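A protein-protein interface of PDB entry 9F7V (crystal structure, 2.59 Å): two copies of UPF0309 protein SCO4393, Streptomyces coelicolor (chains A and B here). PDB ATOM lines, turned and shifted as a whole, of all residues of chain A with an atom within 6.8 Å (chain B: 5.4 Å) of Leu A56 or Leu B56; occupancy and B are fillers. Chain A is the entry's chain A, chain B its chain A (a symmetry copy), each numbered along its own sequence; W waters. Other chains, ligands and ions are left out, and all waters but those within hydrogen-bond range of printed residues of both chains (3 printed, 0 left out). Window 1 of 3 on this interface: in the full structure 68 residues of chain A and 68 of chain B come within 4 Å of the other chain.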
ATOM      1  N   GLY A  50       8.845  -9.924 -20.407  1.00  0.00           N
ATOM      2  CA  GLY A  50       7.853  -9.084 -19.768  1.00  0.00           C
ATOM      3  C   GLY A  50       7.627  -9.569 -18.356  1.00  0.00           C
ATOM      4  O   GLY A  50       7.910 -10.724 -18.023  1.00  0.00           O
ATOM      5  N   ALA A  51       7.112  -8.672 -17.524  1.00  0.00           N
ATOM      6  CA  ALA A  51       6.808  -8.980 -16.136  1.00  0.00           C
ATOM      7  C   ALA A  51       5.319  -9.242 -15.974  1.00  0.00           C
ATOM      8  O   ALA A  51       4.485  -8.622 -16.637  1.00  0.00           O
ATOM      9  CB  ALA A  51       7.244  -7.837 -15.217  1.00  0.00           C
ATOM     10  N   GLY A  52       4.992 -10.158 -15.073  1.00  0.00           N
ATOM     11  CA  GLY A  52       3.598 -10.383 -14.735  1.00  0.00           C
ATOM     12  C   GLY A  52       2.837 -10.795 -15.979  1.00  0.00           C
ATOM     13  O   GLY A  52       3.269 -11.670 -16.734  1.00  0.00           O
ATOM     14  N   HIS A  53       1.678 -10.170 -16.206  1.00  0.00           N
ATOM     15  CA  HIS A  53       0.889 -10.533 -17.375  1.00  0.00           C
ATOM     16  C   HIS A  53       1.547 -10.088 -18.675  1.00  0.00           C
ATOM     17  O   HIS A  53       1.188 -10.596 -19.741  1.00  0.00           O
ATOM     18  CB  HIS A  53      -0.527  -9.967 -17.275  1.00  0.00           C
ATOM     19  CG  HIS A  53      -1.325 -10.554 -16.152  1.00  0.00           C
ATOM     20  ND1 HIS A  53      -1.374  -9.984 -14.900  1.00  0.00           N
ATOM     21  CD2 HIS A  53      -2.038 -11.702 -16.069  1.00  0.00           C
ATOM     22  CE1 HIS A  53      -2.123 -10.727 -14.107  1.00  0.00           C
ATOM     23  NE2 HIS A  53      -2.536 -11.779 -14.791  1.00  0.00           N
ATOM     24  N   SER A  54       2.497  -9.152 -18.617  1.00  0.00           N
ATOM     25  CA  SER A  54       3.246  -8.806 -19.817  1.00  0.00           C
ATOM     26  C   SER A  54       4.186  -9.930 -20.227  1.00  0.00           C
ATOM     27  O   SER A  54       4.586 -10.000 -21.393  1.00  0.00           O
ATOM     28  CB  SER A  54       4.043  -7.517 -19.595  1.00  0.00           C
ATOM     29  OG  SER A  54       3.230  -6.368 -19.769  1.00  0.00           O
ATOM     30  N   SER A  55       4.551 -10.803 -19.289  1.00  0.00           N
ATOM     31  CA  SER A  55       5.288 -12.016 -19.619  1.00  0.00           C
ATOM     32  C   SER A  55       4.536 -12.915 -20.591  1.00  0.00           C
ATOM     33  O   SER A  55       5.169 -13.698 -21.307  1.00  0.00           O
ATOM     34  CB  SER A  55       5.592 -12.799 -18.340  1.00  0.00           C
ATOM     35  OG  SER A  55       6.348 -13.963 -18.619  1.00  0.00           O
ATOM     36  N   LEU A  56       3.210 -12.803 -20.657  1.00  0.00           N
ATOM     37  CA  LEU A  56       2.430 -13.737 -21.461  1.00  0.00           C
ATOM     38  C   LEU A  56       2.617 -13.496 -22.954  1.00  0.00           C
ATOM     39  O   LEU A  56       2.705 -14.451 -23.731  1.00  0.00           O
ATOM     40  CB  LEU A  56       0.952 -13.626 -21.089  1.00  0.00           C
ATOM     41  CG  LEU A  56       0.615 -13.758 -19.599  1.00  0.00           C
ATOM     42  CD1 LEU A  56      -0.878 -13.578 -19.384  1.00  0.00           C
ATOM     43  CD2 LEU A  56       1.082 -15.084 -19.015  1.00  0.00           C
ATOM     44  N   ALA A  57       2.721 -12.233 -23.374  1.00  0.00           N
ATOM     45  CA  ALA A  57       3.010 -11.953 -24.777  1.00  0.00           C
ATOM     46  C   ALA A  57       4.401 -12.434 -25.165  1.00  0.00           C
ATOM     47  O   ALA A  57       4.612 -12.881 -26.300  1.00  0.00           O
ATOM     48  CB  ALA A  57       2.867 -10.458 -25.049  1.00  0.00           C
ATOM     49  N   ALA A  58       5.367 -12.318 -24.254  1.00  0.00           N
ATOM     50  CA  ALA A  58       6.712 -12.817 -24.528  1.00  0.00           C
ATOM     51  C   ALA A  58       6.712 -14.333 -24.682  1.00  0.00           C
ATOM     52  O   ALA A  58       7.320 -14.877 -25.611  1.00  0.00           O
ATOM     53  CB  ALA A  58       7.666 -12.385 -23.416  1.00  0.00           C
ATOM     54  N   GLN A  59       6.034 -15.033 -23.771  1.00  0.00           N
ATOM     55  CA  GLN A  59       5.927 -16.487 -23.853  1.00  0.00           C
ATOM     56  C   GLN A  59       5.215 -16.935 -25.123  1.00  0.00           C
ATOM     57  O   GLN A  59       5.496 -18.022 -25.636  1.00  0.00           O
ATOM     58  CB  GLN A  59       5.208 -17.013 -22.611  1.00  0.00           C
ATOM     59  CG  GLN A  59       5.996 -16.768 -21.333  1.00  0.00           C
ATOM     60  CD  GLN A  59       5.375 -17.414 -20.113  1.00  0.00           C
ATOM     61  OE1 GLN A  59       5.018 -16.730 -19.156  1.00  0.00           O
ATOM     62  NE2 GLN A  59       5.247 -18.728 -20.136  1.00  0.00           N
ATOM     63  N   ASP A  60       4.320 -16.108 -25.663  1.00  0.00           N
ATOM     64  CA  ASP A  60       3.518 -16.532 -26.804  1.00  0.00           C
ATOM     65  C   ASP A  60       4.349 -16.691 -28.074  1.00  0.00           C
ATOM     66  O   ASP A  60       3.873 -17.308 -29.031  1.00  0.00           O
ATOM     67  CB  ASP A  60       2.398 -15.517 -27.055  1.00  0.00           C
ATOM     68  CG  ASP A  60       1.232 -16.101 -27.830  1.00  0.00           C
ATOM     69  OD1 ASP A  60       0.924 -17.298 -27.656  1.00  0.00           O
ATOM     70  OD2 ASP A  60       0.628 -15.355 -28.629  1.00  0.00           O
ATOM     71  N   VAL A  61       5.553 -16.119 -28.123  1.00  0.00           N
ATOM     72  CA  VAL A  61       6.437 -16.256 -29.277  1.00  0.00           C
ATOM     73  C   VAL A  61       7.583 -17.236 -29.027  1.00  0.00           C
ATOM     74  O   VAL A  61       8.467 -17.370 -29.878  1.00  0.00           O
ATOM     75  CB  VAL A  61       6.989 -14.888 -29.710  1.00  0.00           C
ATOM     76  CG1 VAL A  61       5.869 -14.026 -30.270  1.00  0.00           C
ATOM     77  CG2 VAL A  61       7.683 -14.186 -28.542  1.00  0.00           C
ATOM     78  N   ARG A  64       6.859 -21.995 -30.034  1.00  0.00           N
ATOM     79  CA  ARG A  64       5.469 -21.762 -30.391  1.00  0.00           C
ATOM     80  C   ARG A  64       5.180 -22.361 -31.761  1.00  0.00           C
ATOM     81  O   ARG A  64       5.949 -22.159 -32.707  1.00  0.00           O
ATOM     82  CB  ARG A  64       5.177 -20.259 -30.388  1.00  0.00           C
ATOM     83  CG  ARG A  64       3.741 -19.895 -30.657  1.00  0.00           C
ATOM     84  CD  ARG A  64       2.910 -20.225 -29.413  1.00  0.00           C
ATOM     85  NE  ARG A  64       1.648 -19.501 -29.382  1.00  0.00           N
ATOM     86  CZ  ARG A  64       0.510 -19.950 -29.888  1.00  0.00           C
ATOM     87  NH1 ARG A  64       0.465 -21.055 -30.616  1.00  0.00           N
ATOM     88  NH2 ARG A  64      -0.598 -19.230 -29.727  1.00  0.00           N
ATOM     89  N   VAL A  80       7.678 -14.319 -13.889  1.00  0.00           N
ATOM     90  CA  VAL A  80       7.268 -15.074 -15.073  1.00  0.00           C
ATOM     91  C   VAL A  80       5.781 -15.369 -14.911  1.00  0.00           C
ATOM     92  O   VAL A  80       5.392 -16.302 -14.209  1.00  0.00           O
ATOM     93  CB  VAL A  80       8.084 -16.354 -15.257  1.00  0.00           C
ATOM     94  CG1 VAL A  80       7.539 -17.162 -16.426  1.00  0.00           C
ATOM     95  CG2 VAL A  80       9.546 -16.016 -15.491  1.00  0.00           C
ATOM     96  N   GLY A  81       4.943 -14.583 -15.577  1.00  0.00           N
ATOM     97  CA  GLY A  81       3.527 -14.716 -15.337  1.00  0.00           C
ATOM     98  C   GLY A  81       3.208 -14.361 -13.897  1.00  0.00           C
ATOM     99  O   GLY A  81       3.850 -13.505 -13.279  1.00  0.00           O
ATOM    100  N   ILE A  82       2.188 -15.020 -13.355  1.00  0.00           N
ATOM    101  CA  ILE A  82       1.684 -14.718 -12.022  1.00  0.00           C
ATOM    102  C   ILE A  82       1.753 -15.952 -11.128  1.00  0.00           C
ATOM    103  O   ILE A  82       1.053 -16.043 -10.127  1.00  0.00           O
ATOM    104  CB  ILE A  82       0.259 -14.131 -12.075  1.00  0.00           C
ATOM    105  CG1 ILE A  82      -0.665 -14.956 -12.972  1.00  0.00           C
ATOM    106  CG2 ILE A  82       0.307 -12.706 -12.598  1.00  0.00           C
ATOM    107  CD1 ILE A  82      -1.017 -16.308 -12.410  1.00  0.00           C
ATOM    108  N   ILE A 118       8.280  -6.129 -23.106  1.00  0.00           N
ATOM    109  CA  ILE A 118       6.860  -5.815 -23.033  1.00  0.00           C
ATOM    110  C   ILE A 118       6.570  -5.279 -21.639  1.00  0.00           C
ATOM    111  O   ILE A 118       6.805  -5.965 -20.637  1.00  0.00           O
ATOM    112  CB  ILE A 118       5.985  -7.045 -23.331  1.00  0.00           C
ATOM    113  CG1 ILE A 118       6.281  -7.611 -24.721  1.00  0.00           C
ATOM    114  CG2 ILE A 118       4.507  -6.679 -23.226  1.00  0.00           C
ATOM    115  CD1 ILE A 118       6.711  -9.063 -24.706  1.00  0.00           C
ATOM    116  N   THR A 196      -3.506  -8.094 -22.940  1.00  0.00           N
ATOM    117  CA  THR A 196      -2.847  -9.317 -23.381  1.00  0.00           C
ATOM    118  C   THR A 196      -3.291  -9.704 -24.786  1.00  0.00           C
ATOM    119  O   THR A 196      -2.473 -10.137 -25.606  1.00  0.00           O
ATOM    120  CB  THR A 196      -3.119 -10.454 -22.393  1.00  0.00           C
ATOM    121  OG1 THR A 196      -2.628 -10.094 -21.097  1.00  0.00           O
ATOM    122  CG2 THR A 196      -2.428 -11.729 -22.832  1.00  0.00           C
ATOM    123  N   THR A 199      -1.218  -7.202 -26.917  1.00  0.00           N
ATOM    124  CA  THR A 199       0.236  -7.363 -26.949  1.00  0.00           C
ATOM    125  C   THR A 199       0.623  -8.678 -27.610  1.00  0.00           C
ATOM    126  O   THR A 199       1.640  -8.748 -28.312  1.00  0.00           O
ATOM    127  CB  THR A 199       0.838  -7.267 -25.545  1.00  0.00           C
ATOM    128  OG1 THR A 199       0.237  -8.239 -24.680  1.00  0.00           O
ATOM    129  CG2 THR A 199       0.629  -5.866 -24.979  1.00  0.00           C
ATOM    130  N   ALA A 200      -0.168  -9.733 -27.401  1.00  0.00           N
ATOM    131  CA  ALA A 200       0.138 -10.992 -28.067  1.00  0.00           C
ATOM    132  C   ALA A 200       0.059 -10.801 -29.575  1.00  0.00           C
ATOM    133  O   ALA A 200       0.912 -11.295 -30.322  1.00  0.00           O
ATOM    134  CB  ALA A 200      -0.820 -12.090 -27.605  1.00  0.00           C
ATOM    135  N   GLY B  52       0.949 -25.266 -21.150  1.00  0.00           N
ATOM    136  CA  GLY B  52       1.784 -24.625 -22.150  1.00  0.00           C
ATOM    137  C   GLY B  52       1.242 -23.243 -22.451  1.00  0.00           C
ATOM    138  O   GLY B  52       0.936 -22.463 -21.544  1.00  0.00           O
ATOM    139  N   HIS B  53       1.120 -22.916 -23.741  1.00  0.00           N
ATOM    140  CA  HIS B  53       0.622 -21.594 -24.096  1.00  0.00           C
ATOM    141  C   HIS B  53      -0.857 -21.429 -23.768  1.00  0.00           C
ATOM    142  O   HIS B  53      -1.340 -20.294 -23.699  1.00  0.00           O
ATOM    143  CB  HIS B  53       0.875 -21.296 -25.574  1.00  0.00           C
ATOM    144  CG  HIS B  53       2.328 -21.196 -25.920  1.00  0.00           C
ATOM    145  ND1 HIS B  53       3.061 -22.274 -26.363  1.00  0.00           N
ATOM    146  CD2 HIS B  53       3.203 -20.168 -25.811  1.00  0.00           C
ATOM    147  CE1 HIS B  53       4.313 -21.905 -26.561  1.00  0.00           C
ATOM    148  NE2 HIS B  53       4.428 -20.632 -26.229  1.00  0.00           N
ATOM    149  N   SER B  54      -1.589 -22.527 -23.568  1.00  0.00           N
ATOM    150  CA  SER B  54      -2.968 -22.405 -23.113  1.00  0.00           C
ATOM    151  C   SER B  54      -3.034 -21.931 -21.669  1.00  0.00           C
ATOM    152  O   SER B  54      -4.063 -21.392 -21.248  1.00  0.00           O
ATOM    153  CB  SER B  54      -3.696 -23.744 -23.255  1.00  0.00           C
ATOM    154  OG  SER B  54      -4.151 -23.950 -24.582  1.00  0.00           O
ATOM    155  N   SER B  55      -1.962 -22.126 -20.905  1.00  0.00           N
ATOM    156  CA  SER B  55      -1.854 -21.543 -19.574  1.00  0.00           C
ATOM    157  C   SER B  55      -1.938 -20.022 -19.591  1.00  0.00           C
ATOM    158  O   SER B  55      -2.321 -19.424 -18.580  1.00  0.00           O
ATOM    159  CB  SER B  55      -0.533 -21.968 -18.928  1.00  0.00           C
ATOM    160  OG  SER B  55      -0.416 -21.454 -17.615  1.00  0.00           O
ATOM    161  N   LEU B  56      -1.617 -19.385 -20.717  1.00  0.00           N
ATOM    162  CA  LEU B  56      -1.539 -17.929 -20.744  1.00  0.00           C
ATOM    163  C   LEU B  56      -2.917 -17.284 -20.662  1.00  0.00           C
ATOM    164  O   LEU B  56      -3.088 -16.267 -19.984  1.00  0.00           O
ATOM    165  CB  LEU B  56      -0.818 -17.477 -22.013  1.00  0.00           C
ATOM    166  CG  LEU B  56       0.552 -18.113 -22.281  1.00  0.00           C
ATOM    167  CD1 LEU B  56       1.116 -17.602 -23.595  1.00  0.00           C
ATOM    168  CD2 LEU B  56       1.535 -17.867 -21.145  1.00  0.00           C
ATOM    169  N   ALA B  57      -3.922 -17.876 -21.311  1.00  0.00           N
ATOM    170  CA  ALA B  57      -5.281 -17.360 -21.175  1.00  0.00           C
ATOM    171  C   ALA B  57      -5.801 -17.527 -19.755  1.00  0.00           C
ATOM    172  O   ALA B  57      -6.553 -16.678 -19.261  1.00  0.00           O
ATOM    173  CB  ALA B  57      -6.206 -18.061 -22.167  1.00  0.00           C
ATOM    174  N   ALA B  58      -5.441 -18.630 -19.095  1.00  0.00           N
ATOM    175  CA  ALA B  58      -5.845 -18.832 -17.707  1.00  0.00           C
ATOM    176  C   ALA B  58      -5.206 -17.791 -16.795  1.00  0.00           C
ATOM    177  O   ALA B  58      -5.873 -17.204 -15.936  1.00  0.00           O
ATOM    178  CB  ALA B  58      -5.480 -20.244 -17.256  1.00  0.00           C
ATOM    179  N   GLN B  59      -3.904 -17.556 -16.968  1.00  0.00           N
ATOM    180  CA  GLN B  59      -3.204 -16.543 -16.181  1.00  0.00           C
ATOM    181  C   GLN B  59      -3.765 -15.147 -16.421  1.00  0.00           C
ATOM    182  O   GLN B  59      -3.720 -14.302 -15.521  1.00  0.00           O
ATOM    183  CB  GLN B  59      -1.712 -16.592 -16.506  1.00  0.00           C
ATOM    184  CG  GLN B  59      -1.065 -17.904 -16.086  1.00  0.00           C
ATOM    185  CD  GLN B  59       0.438 -17.915 -16.261  1.00  0.00           C
ATOM    186  OE1 GLN B  59       0.977 -18.734 -17.003  1.00  0.00           O
ATOM    187  NE2 GLN B  59       1.123 -17.016 -15.579  1.00  0.00           N
ATOM    188  N   ASP B  60      -4.324 -14.892 -17.603  1.00  0.00           N
ATOM    189  CA  ASP B  60      -4.765 -13.543 -17.934  1.00  0.00           C
ATOM    190  C   ASP B  60      -5.972 -13.104 -17.110  1.00  0.00           C
ATOM    191  O   ASP B  60      -6.274 -11.908 -17.075  1.00  0.00           O
ATOM    192  CB  ASP B  60      -5.115 -13.465 -19.424  1.00  0.00           C
ATOM    193  CG  ASP B  60      -5.064 -12.051 -19.971  1.00  0.00           C
ATOM    194  OD1 ASP B  60      -4.222 -11.251 -19.514  1.00  0.00           O
ATOM    195  OD2 ASP B  60      -5.884 -11.737 -20.859  1.00  0.00           O
ATOM    196  N   GLY B  81       2.788 -22.173 -18.526  1.00  0.00           N
ATOM    197  CA  GLY B  81       3.506 -21.521 -19.592  1.00  0.00           C
ATOM    198  C   GLY B  81       4.584 -22.440 -20.133  1.00  0.00           C
ATOM    199  O   GLY B  81       4.441 -23.667 -20.160  1.00  0.00           O
ATOM    200  N   THR B 196      -3.642 -17.590 -28.790  1.00  0.00           N
ATOM    201  CA  THR B 196      -3.593 -16.894 -27.509  1.00  0.00           C
ATOM    202  C   THR B 196      -4.380 -15.590 -27.564  1.00  0.00           C
ATOM    203  O   THR B 196      -5.084 -15.242 -26.609  1.00  0.00           O
ATOM    204  CB  THR B 196      -2.141 -16.635 -27.100  1.00  0.00           C
ATOM    205  OG1 THR B 196      -1.443 -17.880 -26.986  1.00  0.00           O
ATOM    206  CG2 THR B 196      -2.076 -15.923 -25.765  1.00  0.00           C
HETATM  207  O   HOH W   1      -1.316 -16.030 -30.398  1.00  0.00           O
HETATM  208  O   HOH W   2      -6.333  -9.281 -21.925  1.00  0.00           O
HETATM  209  O   HOH W   3       3.985 -18.468 -16.909  1.00  0.00           O
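Among the printed residues, pairs that only touch across the chains: His A53 with Asp B60, Leu A56 with Leu B56, Leu A56 with Gln B59, Gln A59 with Leu B56, Gln A59 with Gly B81, Asp A60 with His B53, Arg A64 with His B53 and Gly A81 with Gln B59.
Water W1 lies within hydrogen-bond range of the side-chain carboxylate of Asp A60, the backbone NH of Thr B196 and the guanidinium group of Arg A64. Water W2 lies within hydrogen-bond range of the side-chain carboxylate of Asp B60 (2.7 Å) and the backbone NH of Thr A196 (3.2 Å). Water W3 bridges OE1 of Gln B59 and OE1 of Gln A59.
Hydrophobic or aromatic side chains of chain B within 4 Å of the printed part of chain A: His B53 and Leu B56. Printed residues of chain A that touch a printed residue of chain B: His A53, Leu A56, Gln A59, Asp A60, Arg A64, Gly A81, Ile A82 and Thr A196. Hydrophobic or aromatic side chains of chain A within 4 Å of the printed part of chain B: His A53, Leu A56 and Ile A82. Among the printed residues, no Asp or Glu carboxylate lies within 4 Å of a Lys or Arg side-chain nitrogen of the other chain.
His A53 touches Gln B59, and with the chains exchanged Gln A59 touches His B53. His A53 touches Asp B60, and with the chains exchanged Asp A60 touches His B53. Leu A56 touches Gln B59, and with the chains exchanged Gln A59 touches Leu B56. Asp A60 touches Thr B196, and with the chains exchanged Thr A196 touches Asp B60. 11 positions are printed for both chains.
The side-chain carboxylate of Asp A60 lies within hydrogen-bond range of the side-chain hydroxyl of Thr B196 (2.5 Å). The side-chain hydroxyl (OG1) of Thr B196 is in hydrogen-bond range of the guanidinium group (NH2) of Arg A64, at 3.2 Å. NE2 of His A53 lies within hydrogen-bond range of O of Gln B59 (2.9 Å). N of Ile A82 sits close to NE2 of Gln B59. The side-chain carboxylate (OD1) of Asp B60 is in hydrogen-bond range of the side-chain hydroxyl (OG1) of Thr A196 (2.5 Å). NE2 of His B53 is in hydrogen-bond range of O of Gln A59, 2.9 Å away.
The backbone carbonyl oxygen (O) of Thr A196 is in hydrogen-bond range of the side-chain hydroxyl (OG1) of Thr A199 (3.4 Å). OG of Ser A55 lies within hydrogen-bond range of OE1 of Gln A59 (3.1 Å). OG of Ser A55 sits close to N of Gly A81 (3.4 Å). OG of Ser B55 lies within hydrogen-bond range of OE1 of Gln B59 (3.1 Å). The side-chain carboxylate (OD1) of Asp A60 is in salt-bridge range of the guanidinium group (NE) of Arg A64 (2.9 Å). N of Gly B81 lies close to OG of Ser B55, 3.4 Å away.
Ser A54 touches none of the printed residues of chain B. Leu A56 touches just these residues of chain B: Leu B56 and Gln B59. Printed residues of chain B within 4 Å of Gln A59: His B53, Leu B56 and Gly B81. Printed residues of chain B within 4 Å of Gly A81: Gln B59. Ile A118 touches none of the printed residues of chain B. Leu B56 touches just these residues of chain A: Leu A56 (3.5 Å) and Gln A59 (3.9 Å). The nearest residue of chain B that does not touch Leu A56 is Asp B60 (4.1 Å). The nearest printed residue of chain A that does not touch Asp B60 is Leu A56 (4.1 Å).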
